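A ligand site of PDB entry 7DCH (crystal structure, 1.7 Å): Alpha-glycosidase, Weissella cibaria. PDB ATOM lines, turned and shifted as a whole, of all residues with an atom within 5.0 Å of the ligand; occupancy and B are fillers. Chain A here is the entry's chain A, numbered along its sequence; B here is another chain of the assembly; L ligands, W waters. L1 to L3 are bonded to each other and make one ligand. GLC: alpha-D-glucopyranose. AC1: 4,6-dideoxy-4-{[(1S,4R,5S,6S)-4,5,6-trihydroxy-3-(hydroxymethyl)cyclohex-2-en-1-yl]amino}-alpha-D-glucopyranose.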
ATOM      1  N   ARG A 176      23.200   9.006  26.007  1.00  0.00           N
ATOM      2  CA  ARG A 176      22.388  10.023  25.346  1.00  0.00           C
ATOM      3  C   ARG A 176      22.493   9.934  23.833  1.00  0.00           C
ATOM      4  O   ARG A 176      21.535  10.274  23.117  1.00  0.00           O
ATOM      5  CB  ARG A 176      22.797  11.424  25.811  1.00  0.00           C
ATOM      6  CG  ARG A 176      22.605  11.695  27.312  1.00  0.00           C
ATOM      7  CD  ARG A 176      23.947  11.907  28.049  1.00  0.00           C
ATOM      8  NE  ARG A 176      24.650  10.656  28.365  1.00  0.00           N
ATOM      9  CZ  ARG A 176      25.833  10.306  27.874  1.00  0.00           C
ATOM     10  NH1 ARG A 176      26.491  11.127  27.059  1.00  0.00           N
ATOM     11  NH2 ARG A 176      26.384   9.157  28.224  1.00  0.00           N
ATOM     12  N   HIS A 214      16.389  10.697  19.227  1.00  0.00           N
ATOM     13  CA  HIS A 214      15.025  10.997  19.638  1.00  0.00           C
ATOM     14  C   HIS A 214      14.248  11.831  18.607  1.00  0.00           C
ATOM     15  O   HIS A 214      13.015  11.752  18.576  1.00  0.00           O
ATOM     16  CB  HIS A 214      15.052  11.745  20.962  1.00  0.00           C
ATOM     17  CG  HIS A 214      15.924  12.948  20.942  1.00  0.00           C
ATOM     18  ND1 HIS A 214      15.521  14.149  20.397  1.00  0.00           N
ATOM     19  CD2 HIS A 214      17.170  13.153  21.440  1.00  0.00           C
ATOM     20  CE1 HIS A 214      16.500  15.032  20.531  1.00  0.00           C
ATOM     21  NE2 HIS A 214      17.499  14.455  21.175  1.00  0.00           N
ATOM     22  N   TYR A 216      13.685  15.012  18.147  1.00  0.00           N
ATOM     23  CA  TYR A 216      12.993  16.258  18.445  1.00  0.00           C
ATOM     24  C   TYR A 216      13.732  17.489  17.955  1.00  0.00           C
ATOM     25  O   TYR A 216      13.235  18.611  18.123  1.00  0.00           O
ATOM     26  CB  TYR A 216      12.733  16.375  19.956  1.00  0.00           C
ATOM     27  CG  TYR A 216      11.597  15.498  20.437  1.00  0.00           C
ATOM     28  CD1 TYR A 216      10.293  15.992  20.461  1.00  0.00           C
ATOM     29  CD2 TYR A 216      11.834  14.200  20.904  1.00  0.00           C
ATOM     30  CE1 TYR A 216       9.248  15.216  20.934  1.00  0.00           C
ATOM     31  CE2 TYR A 216      10.797  13.419  21.377  1.00  0.00           C
ATOM     32  CZ  TYR A 216       9.507  13.930  21.382  1.00  0.00           C
ATOM     33  OH  TYR A 216       8.477  13.154  21.836  1.00  0.00           O
ATOM     34  N   VAL A 253       6.413  18.320  16.357  1.00  0.00           N
ATOM     35  CA  VAL A 253       7.366  19.087  17.148  1.00  0.00           C
ATOM     36  C   VAL A 253       7.421  20.466  16.532  1.00  0.00           C
ATOM     37  O   VAL A 253       8.325  20.770  15.739  1.00  0.00           O
ATOM     38  CB  VAL A 253       8.750  18.405  17.157  1.00  0.00           C
ATOM     39  CG1 VAL A 253       9.711  19.075  18.131  1.00  0.00           C
ATOM     40  CG2 VAL A 253       8.604  16.904  17.482  1.00  0.00           C
ATOM     41  N   HIS A 256       9.835  24.253  18.161  1.00  0.00           N
ATOM     42  CA  HIS A 256      11.196  24.548  17.785  1.00  0.00           C
ATOM     43  C   HIS A 256      11.580  23.618  16.654  1.00  0.00           C
ATOM     44  O   HIS A 256      10.926  22.601  16.405  1.00  0.00           O
ATOM     45  CB  HIS A 256      12.134  24.356  18.978  1.00  0.00           C
ATOM     46  CG  HIS A 256      11.854  23.102  19.764  1.00  0.00           C
ATOM     47  ND1 HIS A 256      11.000  23.083  20.853  1.00  0.00           N
ATOM     48  CD2 HIS A 256      12.326  21.836  19.618  1.00  0.00           C
ATOM     49  CE1 HIS A 256      10.941  21.847  21.330  1.00  0.00           C
ATOM     50  NE2 HIS A 256      11.764  21.082  20.617  1.00  0.00           N
ATOM     51  N   ASN A 294      28.338  20.858  28.208  1.00  0.00           N
ATOM     52  CA  ASN A 294      27.064  20.170  28.093  1.00  0.00           C
ATOM     53  C   ASN A 294      26.456  20.557  26.743  1.00  0.00           C
ATOM     54  O   ASN A 294      26.120  21.724  26.533  1.00  0.00           O
ATOM     55  CB  ASN A 294      26.148  20.573  29.250  1.00  0.00           C
ATOM     56  CG  ASN A 294      24.787  19.910  29.183  1.00  0.00           C
ATOM     57  OD1 ASN A 294      24.453  19.219  28.217  1.00  0.00           O
ATOM     58  ND2 ASN A 294      23.983  20.116  30.234  1.00  0.00           N
ATOM     59  N   GLU A 296      23.656  20.219  25.599  1.00  0.00           N
ATOM     60  CA  GLU A 296      22.276  20.690  25.699  1.00  0.00           C
ATOM     61  C   GLU A 296      22.128  22.039  26.412  1.00  0.00           C
ATOM     62  O   GLU A 296      20.994  22.457  26.675  1.00  0.00           O
ATOM     63  CB  GLU A 296      21.419  19.647  26.423  1.00  0.00           C
ATOM     64  CG  GLU A 296      21.567  18.228  25.929  1.00  0.00           C
ATOM     65  CD  GLU A 296      20.813  17.971  24.647  1.00  0.00           C
ATOM     66  OE1 GLU A 296      20.490  18.943  23.942  1.00  0.00           O
ATOM     67  OE2 GLU A 296      20.529  16.786  24.351  1.00  0.00           O
ATOM     68  N   PHE A 306      14.128  26.102  22.854  1.00  0.00           N
ATOM     69  CA  PHE A 306      13.610  25.190  23.854  1.00  0.00           C
ATOM     70  C   PHE A 306      14.571  25.178  25.041  1.00  0.00           C
ATOM     71  O   PHE A 306      15.787  25.108  24.845  1.00  0.00           O
ATOM     72  CB  PHE A 306      13.466  23.765  23.327  1.00  0.00           C
ATOM     73  CG  PHE A 306      13.045  22.808  24.395  1.00  0.00           C
ATOM     74  CD1 PHE A 306      11.766  22.888  24.925  1.00  0.00           C
ATOM     75  CD2 PHE A 306      13.931  21.868  24.903  1.00  0.00           C
ATOM     76  CE1 PHE A 306      11.352  22.030  25.932  1.00  0.00           C
ATOM     77  CE2 PHE A 306      13.530  20.998  25.939  1.00  0.00           C
ATOM     78  CZ  PHE A 306      12.212  21.091  26.451  1.00  0.00           C
ATOM     79  N   THR A 309      18.739  24.979  25.313  1.00  0.00           N
ATOM     80  CA  THR A 309      19.606  24.260  24.378  1.00  0.00           C
ATOM     81  C   THR A 309      19.755  25.047  23.082  1.00  0.00           C
ATOM     82  O   THR A 309      18.765  25.319  22.404  1.00  0.00           O
ATOM     83  CB  THR A 309      19.106  22.858  24.059  1.00  0.00           C
ATOM     84  OG1 THR A 309      19.861  22.396  22.925  1.00  0.00           O
ATOM     85  CG2 THR A 309      17.642  22.817  23.725  1.00  0.00           C
ATOM     86  N   MET A 312      18.025  23.893  19.451  1.00  0.00           N
ATOM     87  CA  MET A 312      16.577  23.889  19.240  1.00  0.00           C
ATOM     88  C   MET A 312      16.046  25.311  19.262  1.00  0.00           C
ATOM     89  O   MET A 312      15.275  25.687  20.150  1.00  0.00           O
ATOM     90  CB  MET A 312      15.877  23.028  20.299  1.00  0.00           C
ATOM     91  CG  MET A 312      16.215  21.541  20.175  1.00  0.00           C
ATOM     92  SD  MET A 312      15.393  20.563  21.438  1.00  0.00           S
ATOM     93  CE  MET A 312      15.686  18.913  20.757  1.00  0.00           C
ATOM     94  N   ARG A 343      -0.021  14.250  18.342  1.00  0.00           N
ATOM     95  CA  ARG A 343       0.459  14.601  19.680  1.00  0.00           C
ATOM     96  C   ARG A 343       1.367  15.818  19.530  1.00  0.00           C
ATOM     97  O   ARG A 343       2.289  15.810  18.703  1.00  0.00           O
ATOM     98  CB  ARG A 343       1.168  13.416  20.325  1.00  0.00           C
ATOM     99  CG  ARG A 343       1.759  13.663  21.767  1.00  0.00           C
ATOM    100  CD  ARG A 343       3.187  14.188  21.745  1.00  0.00           C
ATOM    101  NE  ARG A 343       3.885  14.008  23.025  1.00  0.00           N
ATOM    102  CZ  ARG A 343       5.054  14.568  23.331  1.00  0.00           C
ATOM    103  NH1 ARG A 343       5.662  15.346  22.437  1.00  0.00           N
ATOM    104  NH2 ARG A 343       5.617  14.349  24.516  1.00  0.00           N
ATOM    105  N   ASP A 345       4.046  18.360  20.712  1.00  0.00           N
ATOM    106  CA  ASP A 345       5.171  18.575  21.623  1.00  0.00           C
ATOM    107  C   ASP A 345       5.220  20.009  22.147  1.00  0.00           C
ATOM    108  O   ASP A 345       5.055  20.966  21.382  1.00  0.00           O
ATOM    109  CB  ASP A 345       6.455  18.258  20.868  1.00  0.00           C
ATOM    110  CG  ASP A 345       7.675  18.233  21.763  1.00  0.00           C
ATOM    111  OD1 ASP A 345       7.653  17.456  22.746  1.00  0.00           O
ATOM    112  OD2 ASP A 345       8.663  18.937  21.446  1.00  0.00           O
ATOM    113  N   VAL A 346       5.512  20.160  23.452  1.00  0.00           N
ATOM    114  CA  VAL A 346       5.606  21.474  24.121  1.00  0.00           C
ATOM    115  C   VAL A 346       4.484  22.408  23.657  1.00  0.00           C
ATOM    116  O   VAL A 346       4.708  23.583  23.333  1.00  0.00           O
ATOM    117  CB  VAL A 346       6.978  22.128  23.875  1.00  0.00           C
ATOM    118  CG1 VAL A 346       7.259  23.104  25.027  1.00  0.00           C
ATOM    119  CG2 VAL A 346       8.085  21.101  23.758  1.00  0.00           C
ATOM    120  N   ASN A 348       2.110  24.041  24.944  1.00  0.00           N
ATOM    121  CA  ASN A 348       1.717  25.224  25.688  1.00  0.00           C
ATOM    122  C   ASN A 348       2.539  26.444  25.299  1.00  0.00           C
ATOM    123  O   ASN A 348       2.099  27.567  25.546  1.00  0.00           O
ATOM    124  CB  ASN A 348       1.865  24.947  27.180  1.00  0.00           C
ATOM    125  CG  ASN A 348       3.266  24.433  27.558  1.00  0.00           C
ATOM    126  OD1 ASN A 348       4.031  23.910  26.751  1.00  0.00           O
ATOM    127  ND2 ASN A 348       3.562  24.521  28.840  1.00  0.00           N
ATOM    128  N   GLU A 349       3.691  26.250  24.659  1.00  0.00           N
ATOM    129  CA  GLU A 349       4.565  27.368  24.346  1.00  0.00           C
ATOM    130  C   GLU A 349       4.315  27.917  22.941  1.00  0.00           C
ATOM    131  O   GLU A 349       5.040  28.824  22.506  1.00  0.00           O
ATOM    132  CB  GLU A 349       6.040  26.948  24.585  1.00  0.00           C
ATOM    133  CG  GLU A 349       6.282  26.679  26.081  1.00  0.00           C
ATOM    134  CD  GLU A 349       7.722  26.246  26.437  1.00  0.00           C
ATOM    135  OE1 GLU A 349       8.651  26.446  25.602  1.00  0.00           O
ATOM    136  OE2 GLU A 349       7.911  25.712  27.557  1.00  0.00           O
ATOM    137  N   GLN A 374       0.791  18.124  24.630  1.00  0.00           N
ATOM    138  CA  GLN A 374       1.675  17.718  25.712  1.00  0.00           C
ATOM    139  C   GLN A 374       1.890  18.922  26.627  1.00  0.00           C
ATOM    140  O   GLN A 374       2.704  19.799  26.329  1.00  0.00           O
ATOM    141  CB  GLN A 374       3.013  17.190  25.214  1.00  0.00           C
ATOM    142  CG  GLN A 374       3.866  16.621  26.375  1.00  0.00           C
ATOM    143  CD  GLN A 374       5.341  16.911  26.225  1.00  0.00           C
ATOM    144  OE1 GLN A 374       5.731  17.708  25.378  1.00  0.00           O
ATOM    145  NE2 GLN A 374       6.170  16.283  27.047  1.00  0.00           N
ATOM    146  N   TRP A 376       2.109  19.795  30.967  1.00  0.00           N
ATOM    147  CA  TRP A 376       2.211  19.246  32.333  1.00  0.00           C
ATOM    148  C   TRP A 376       1.310  19.947  33.349  1.00  0.00           C
ATOM    149  O   TRP A 376       1.008  19.356  34.389  1.00  0.00           O
ATOM    150  CB  TRP A 376       3.661  19.352  32.810  1.00  0.00           C
ATOM    151  CG  TRP A 376       4.558  18.267  32.318  1.00  0.00           C
ATOM    152  CD1 TRP A 376       5.152  18.176  31.096  1.00  0.00           C
ATOM    153  CD2 TRP A 376       5.010  17.138  33.077  1.00  0.00           C
ATOM    154  NE1 TRP A 376       5.946  17.030  31.047  1.00  0.00           N
ATOM    155  CE2 TRP A 376       5.859  16.376  32.246  1.00  0.00           C
ATOM    156  CE3 TRP A 376       4.761  16.683  34.376  1.00  0.00           C
ATOM    157  CZ2 TRP A 376       6.482  15.199  32.675  1.00  0.00           C
ATOM    158  CZ3 TRP A 376       5.369  15.519  34.804  1.00  0.00           C
ATOM    159  CH2 TRP A 376       6.212  14.780  33.958  1.00  0.00           C
ATOM    160  N   HIS A 439       8.914   8.213  27.622  1.00  0.00           N
ATOM    161  CA  HIS A 439      10.303   8.374  27.211  1.00  0.00           C
ATOM    162  C   HIS A 439      10.982   9.487  27.956  1.00  0.00           C
ATOM    163  O   HIS A 439      12.155   9.732  27.699  1.00  0.00           O
ATOM    164  CB  HIS A 439      10.371   8.667  25.716  1.00  0.00           C
ATOM    165  CG  HIS A 439       9.626   9.905  25.324  1.00  0.00           C
ATOM    166  ND1 HIS A 439       8.284  10.081  25.579  1.00  0.00           N
ATOM    167  CD2 HIS A 439      10.045  11.034  24.723  1.00  0.00           C
ATOM    168  CE1 HIS A 439       7.906  11.262  25.128  1.00  0.00           C
ATOM    169  NE2 HIS A 439       8.959  11.860  24.595  1.00  0.00           N
ATOM    170  N   ASP A 440      10.252  10.180  28.835  1.00  0.00           N
ATOM    171  CA  ASP A 440      10.844  11.279  29.578  1.00  0.00           C
ATOM    172  C   ASP A 440      11.042  10.966  31.046  1.00  0.00           C
ATOM    173  O   ASP A 440      11.926  11.555  31.668  1.00  0.00           O
ATOM    174  CB  ASP A 440       9.979  12.542  29.457  1.00  0.00           C
ATOM    175  CG  ASP A 440      10.014  13.168  28.066  1.00  0.00           C
ATOM    176  OD1 ASP A 440      11.049  13.078  27.366  1.00  0.00           O
ATOM    177  OD2 ASP A 440       8.983  13.751  27.669  1.00  0.00           O
ATOM    178  N   ASP A 484      15.342   9.393  31.350  1.00  0.00           N
ATOM    179  CA  ASP A 484      16.004   9.597  30.058  1.00  0.00           C
ATOM    180  C   ASP A 484      17.493   9.866  30.244  1.00  0.00           C
ATOM    181  O   ASP A 484      17.848  10.817  30.962  1.00  0.00           O
ATOM    182  CB  ASP A 484      15.288  10.767  29.361  1.00  0.00           C
ATOM    183  CG  ASP A 484      16.030  11.336  28.165  1.00  0.00           C
ATOM    184  OD1 ASP A 484      16.891  10.653  27.572  1.00  0.00           O
ATOM    185  OD2 ASP A 484      15.749  12.505  27.797  1.00  0.00           O
ATOM    186  N   PRO A 485      18.407   9.096  29.598  1.00  0.00           N
ATOM    187  CA  PRO A 485      18.162   8.099  28.549  1.00  0.00           C
ATOM    188  C   PRO A 485      17.886   6.674  28.996  1.00  0.00           C
ATOM    189  O   PRO A 485      17.703   5.784  28.157  1.00  0.00           O
ATOM    190  CB  PRO A 485      19.483   8.106  27.756  1.00  0.00           C
ATOM    191  CG  PRO A 485      20.522   8.394  28.823  1.00  0.00           C
ATOM    192  CD  PRO A 485      19.844   9.408  29.751  1.00  0.00           C
ATOM    193  N   ARG A 488      14.888   4.396  27.847  1.00  0.00           N
ATOM    194  CA  ARG A 488      14.810   4.160  26.416  1.00  0.00           C
ATOM    195  C   ARG A 488      15.621   2.925  26.018  1.00  0.00           C
ATOM    196  O   ARG A 488      16.267   2.909  24.967  1.00  0.00           O
ATOM    197  CB  ARG A 488      15.282   5.386  25.631  1.00  0.00           C
ATOM    198  CG  ARG A 488      14.376   6.589  25.846  1.00  0.00           C
ATOM    199  CD  ARG A 488      15.065   7.887  25.487  1.00  0.00           C
ATOM    200  NE  ARG A 488      14.194   9.022  25.840  1.00  0.00           N
ATOM    201  CZ  ARG A 488      14.387  10.258  25.407  1.00  0.00           C
ATOM    202  NH1 ARG A 488      15.413  10.519  24.578  1.00  0.00           N
ATOM    203  NH2 ARG A 488      13.541  11.213  25.773  1.00  0.00           N
ATOM    204  N   TYR B  46      12.365  27.005  33.358  1.00  0.00           N
ATOM    205  CA  TYR B  46      13.504  26.173  33.022  1.00  0.00           C
ATOM    206  C   TYR B  46      14.759  26.572  33.782  1.00  0.00           C
ATOM    207  O   TYR B  46      15.725  25.798  33.862  1.00  0.00           O
ATOM    208  CB  TYR B  46      13.754  26.258  31.515  1.00  0.00           C
ATOM    209  CG  TYR B  46      12.649  25.647  30.668  1.00  0.00           C
ATOM    210  CD1 TYR B  46      12.695  24.297  30.342  1.00  0.00           C
ATOM    211  CD2 TYR B  46      11.584  26.407  30.199  1.00  0.00           C
ATOM    212  CE1 TYR B  46      11.704  23.698  29.579  1.00  0.00           C
ATOM    213  CE2 TYR B  46      10.574  25.832  29.428  1.00  0.00           C
ATOM    214  CZ  TYR B  46      10.648  24.486  29.112  1.00  0.00           C
ATOM    215  OH  TYR B  46       9.680  23.898  28.331  1.00  0.00           O
ATOM    216  N   ARG B  49      16.128  23.951  36.855  1.00  0.00           N
ATOM    217  CA  ARG B  49      16.918  22.774  36.478  1.00  0.00           C
ATOM    218  C   ARG B  49      18.177  23.164  35.700  1.00  0.00           C
ATOM    219  O   ARG B  49      19.243  22.568  35.895  1.00  0.00           O
ATOM    220  CB  ARG B  49      16.049  21.797  35.642  1.00  0.00           C
ATOM    221  CG  ARG B  49      15.603  22.177  34.132  1.00  0.00           C
ATOM    222  CD  ARG B  49      14.473  21.208  33.565  1.00  0.00           C
ATOM    223  NE  ARG B  49      14.354  21.211  32.099  1.00  0.00           N
ATOM    224  CZ  ARG B  49      13.457  20.510  31.380  1.00  0.00           C
ATOM    225  NH1 ARG B  49      12.555  19.738  31.970  1.00  0.00           N
ATOM    226  NH2 ARG B  49      13.470  20.604  30.053  1.00  0.00           N
ATOM    227  N   MET B 119       9.557  22.571  38.055  1.00  0.00           N
ATOM    228  CA  MET B 119       8.823  23.598  37.325  1.00  0.00           C
ATOM    229  C   MET B 119       7.353  23.251  37.239  1.00  0.00           C
ATOM    230  O   MET B 119       6.509  24.149  37.134  1.00  0.00           O
ATOM    231  CB  MET B 119       9.408  23.819  35.924  1.00  0.00           C
ATOM    232  CG  MET B 119       9.573  22.560  35.087  1.00  0.00           C
ATOM    233  SD  MET B 119      10.476  22.931  33.542  1.00  0.00           S
ATOM    234  CE  MET B 119       9.141  23.448  32.516  1.00  0.00           C
ATOM    235  N   ASN B 120       7.013  21.960  37.318  1.00  0.00           N
ATOM    236  CA  ASN B 120       5.614  21.578  37.133  1.00  0.00           C
ATOM    237  C   ASN B 120       4.769  21.774  38.392  1.00  0.00           C
ATOM    238  O   ASN B 120       3.549  21.561  38.346  1.00  0.00           O
ATOM    239  CB  ASN B 120       5.564  20.131  36.644  1.00  0.00           C
ATOM    240  CG  ASN B 120       6.234  19.990  35.280  1.00  0.00           C
ATOM    241  OD1 ASN B 120       6.085  20.862  34.451  1.00  0.00           O
ATOM    242  ND2 ASN B 120       6.975  18.902  35.070  1.00  0.00           N
HETATM  243  C1  GLC L   1       9.172  20.333  29.755  1.00  0.00           C
HETATM  244  C2  GLC L   1       8.345  20.558  28.475  1.00  0.00           C
HETATM  245  C3  GLC L   1       8.102  19.286  27.712  1.00  0.00           C
HETATM  246  C4  GLC L   1       9.405  18.634  27.370  1.00  0.00           C
HETATM  247  C5  GLC L   1      10.189  18.370  28.658  1.00  0.00           C
HETATM  248  C6  GLC L   1      11.528  17.790  28.380  1.00  0.00           C
HETATM  249  O1  GLC L   1       8.451  19.536  30.621  1.00  0.00           O
HETATM  250  O2  GLC L   1       7.075  21.169  28.805  1.00  0.00           O
HETATM  251  O3  GLC L   1       7.334  19.616  26.527  1.00  0.00           O
HETATM  252  O4  GLC L   1       9.257  17.326  26.774  1.00  0.00           O
HETATM  253  O5  GLC L   1      10.433  19.600  29.463  1.00  0.00           O
HETATM  254  O6  GLC L   1      12.054  17.484  29.644  1.00  0.00           O
HETATM  255  C1  GLC L   2       9.038  17.279  25.416  1.00  0.00           C
HETATM  256  C2  GLC L   2       9.310  15.868  24.887  1.00  0.00           C
HETATM  257  C3  GLC L   2      10.761  15.570  25.155  1.00  0.00           C
HETATM  258  C4  GLC L   2      11.650  16.442  24.318  1.00  0.00           C
HETATM  259  C5  GLC L   2      11.367  17.923  24.605  1.00  0.00           C
HETATM  260  C6  GLC L   2      11.937  18.828  23.546  1.00  0.00           C
HETATM  261  O2  GLC L   2       8.409  14.956  25.537  1.00  0.00           O
HETATM  262  O3  GLC L   2      11.032  14.158  24.890  1.00  0.00           O
HETATM  263  O4  GLC L   2      12.991  16.161  24.687  1.00  0.00           O
HETATM  264  O5  GLC L   2       9.911  18.211  24.699  1.00  0.00           O
HETATM  265  O6  GLC L   2      11.333  18.588  22.288  1.00  0.00           O
HETATM  266  C1  AC1 L   3      13.842  15.833  23.624  1.00  0.00           C
HETATM  267  O2  AC1 L   3      13.560  13.512  24.085  1.00  0.00           O
HETATM  268  C2  AC1 L   3      14.558  14.534  23.955  1.00  0.00           C
HETATM  269  C4A AC1 L   3      18.451  15.645  29.929  1.00  0.00           C
HETATM  270  C3  AC1 L   3      15.365  14.658  25.204  1.00  0.00           C
HETATM  271  O3  AC1 L   3      16.176  13.438  25.305  1.00  0.00           O
HETATM  272  C4  AC1 L   3      16.293  15.821  25.083  1.00  0.00           C
HETATM  273  N4A AC1 L   3      17.233  15.960  26.249  1.00  0.00           N
HETATM  274  C5  AC1 L   3      15.559  17.144  24.730  1.00  0.00           C
HETATM  275  O5  AC1 L   3      14.787  16.932  23.475  1.00  0.00           O
HETATM  276  C6  AC1 L   3      16.517  18.263  24.483  1.00  0.00           C
HETATM  277  C1B AC1 L   3      16.741  16.374  27.548  1.00  0.00           C
HETATM  278  C2B AC1 L   3      17.911  17.421  28.185  1.00  0.00           C
HETATM  279  O2B AC1 L   3      18.478  18.150  27.058  1.00  0.00           O
HETATM  280  C3B AC1 L   3      18.921  16.861  28.837  1.00  0.00           C
HETATM  281  O3B AC1 L   3      19.682  17.867  29.583  1.00  0.00           O
HETATM  282  O4  AC1 L   3      19.558  15.127  30.586  1.00  0.00           O
HETATM  283  C5B AC1 L   3      17.828  14.635  29.163  1.00  0.00           C
HETATM  284  C7B AC1 L   3      16.567  15.196  28.361  1.00  0.00           C
HETATM  285  C6B AC1 L   3      18.785  13.651  28.468  1.00  0.00           C
HETATM  286  O6B AC1 L   3      19.310  14.272  27.319  1.00  0.00           O
HETATM  287  O   HOH W   1       6.472  23.782  29.082  1.00  0.00           O
HETATM  288  O   HOH W   2      13.464  14.018  28.515  1.00  0.00           O
HETATM  289  O   HOH W   3       6.415  21.449  31.804  1.00  0.00           O
HETATM  290  O   HOH W   4       8.178  15.690  29.380  1.00  0.00           O
HETATM  291  O   HOH W   5       4.070  21.627  30.298  1.00  0.00           O
HETATM  292  O   HOH W   6       9.284  18.573  32.909  1.00  0.00           O
HETATM  293  O   HOH W   7       4.720  21.333  27.560  1.00  0.00           O
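An oxygen (O5) of GLC L1 lies within hydrogen-bond range of the guanidinium group (NH2) of Arg 49 of chain B (3.3 Å). An oxygen (O2) of GLC L2 is in hydrogen-bond range of the guanidinium group of Arg 343 (3.0 Å). The side-chain carboxylate of Asp 484 is in hydrogen-bond range of an oxygen (O3) of AC1 L3 (2.7 Å). The side-chain carboxylate of Asp 345 lies within hydrogen-bond range of an oxygen (O6) of GLC L2 (2.8 Å). NE2 of His 439 sits at hydrogen-bond distance from O3 of GLC L2. The side-chain carboxylate of Asp 440 is in hydrogen-bond range of an oxygen (O2) of GLC L2 (2.5 Å). OE2 of Glu 296 lies within salt-bridge range of N4A of AC1 L3 (3.9 Å). NH2 of Arg 488 sits at hydrogen-bond distance from O2 of AC1 L3, at 2.9 Å. NE2 of His 256 is in hydrogen-bond range of O6 of GLC L2, at 3.0 Å. The side-chain amide oxygen (OE1) of Gln 374 sits at hydrogen-bond distance from an oxygen (O3) of GLC L1, at 2.7 Å.
A ring nitrogen (NE2) of His 439 is in hydrogen-bond range of the side-chain hydroxyl (OH) of Tyr 216, 3.1 Å away. OD1 of Asp 345 lies within salt-bridge range of NH1 of Arg 343. N of Glu 296 is in hydrogen-bond range of OD1 of Asn 294 (2.9 Å). The side-chain amide nitrogen of Gln 374 sits close to the guanidinium group of Arg 343 (3.2 Å). The side-chain hydroxyl (OH) of Tyr 46 of chain B lies within hydrogen-bond range of the side-chain carboxylate (OE2) of Glu 349. OD1 of Asp 345 sits close to OE1 of Gln 374, 3.3 Å away. A ring nitrogen (NE2) of His 256 is in hydrogen-bond range of the side-chain sulfur of Met 312 (3.8 Å). N of Tyr 216 sits at hydrogen-bond distance from ND1 of His 214 (3.0 Å).
Residues that only touch the ligand: His 214 (3.7 Å), Tyr 216 (3.3 Å), Phe 306 (3.6 Å), Met 312 (3.5 Å), Val 346 (3.2 Å), Trp 376 (3.6 Å) and Tyr 46 of chain B (3.6 Å). Hydrophobic or aromatic side chains within 4 Å of the ligand: His 214, Tyr 216, His 256, Phe 306, Met 312, Val 346, Trp 376 and His 439. Within 4 Å of the ligand: His 214, Tyr 216, His 256, Glu 296, Phe 306, Met 312, Arg 343, Asp 345, Val 346, Gln 374, Trp 376, His 439, Asp 440, Asp 484, Arg 488, Tyr 46 of chain B and Arg 49 of chain B.
Water W6 lies within hydrogen-bond range of O1 of GLC L1 (2.6 Å) and ND2 of Asn 120 of chain B (3.2 Å). Water W7 lies within hydrogen-bond range of O2 of GLC L1 (2.7 Å), OD1 of Asn 348 (2.8 Å) and O of Gln 374 (2.8 Å). Water W3 lies within hydrogen-bond range of the side-chain amide oxygen of Asn 120 of chain B and an oxygen (O1) of GLC L1. Water W4 lies within hydrogen-bond range of OD2 of Asp 440, NE1 of Trp 376, NE2 of Gln 374 and O4 of GLC L1. Water W2 bridges OD2 of Asp 484 and OD1 of Asp 440. Water W5 lies within hydrogen-bond range of N of Trp 376 (2.8 Å), ND2 of Asn 348 (3.3 Å) and O2 of GLC L1 (3.4 Å).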
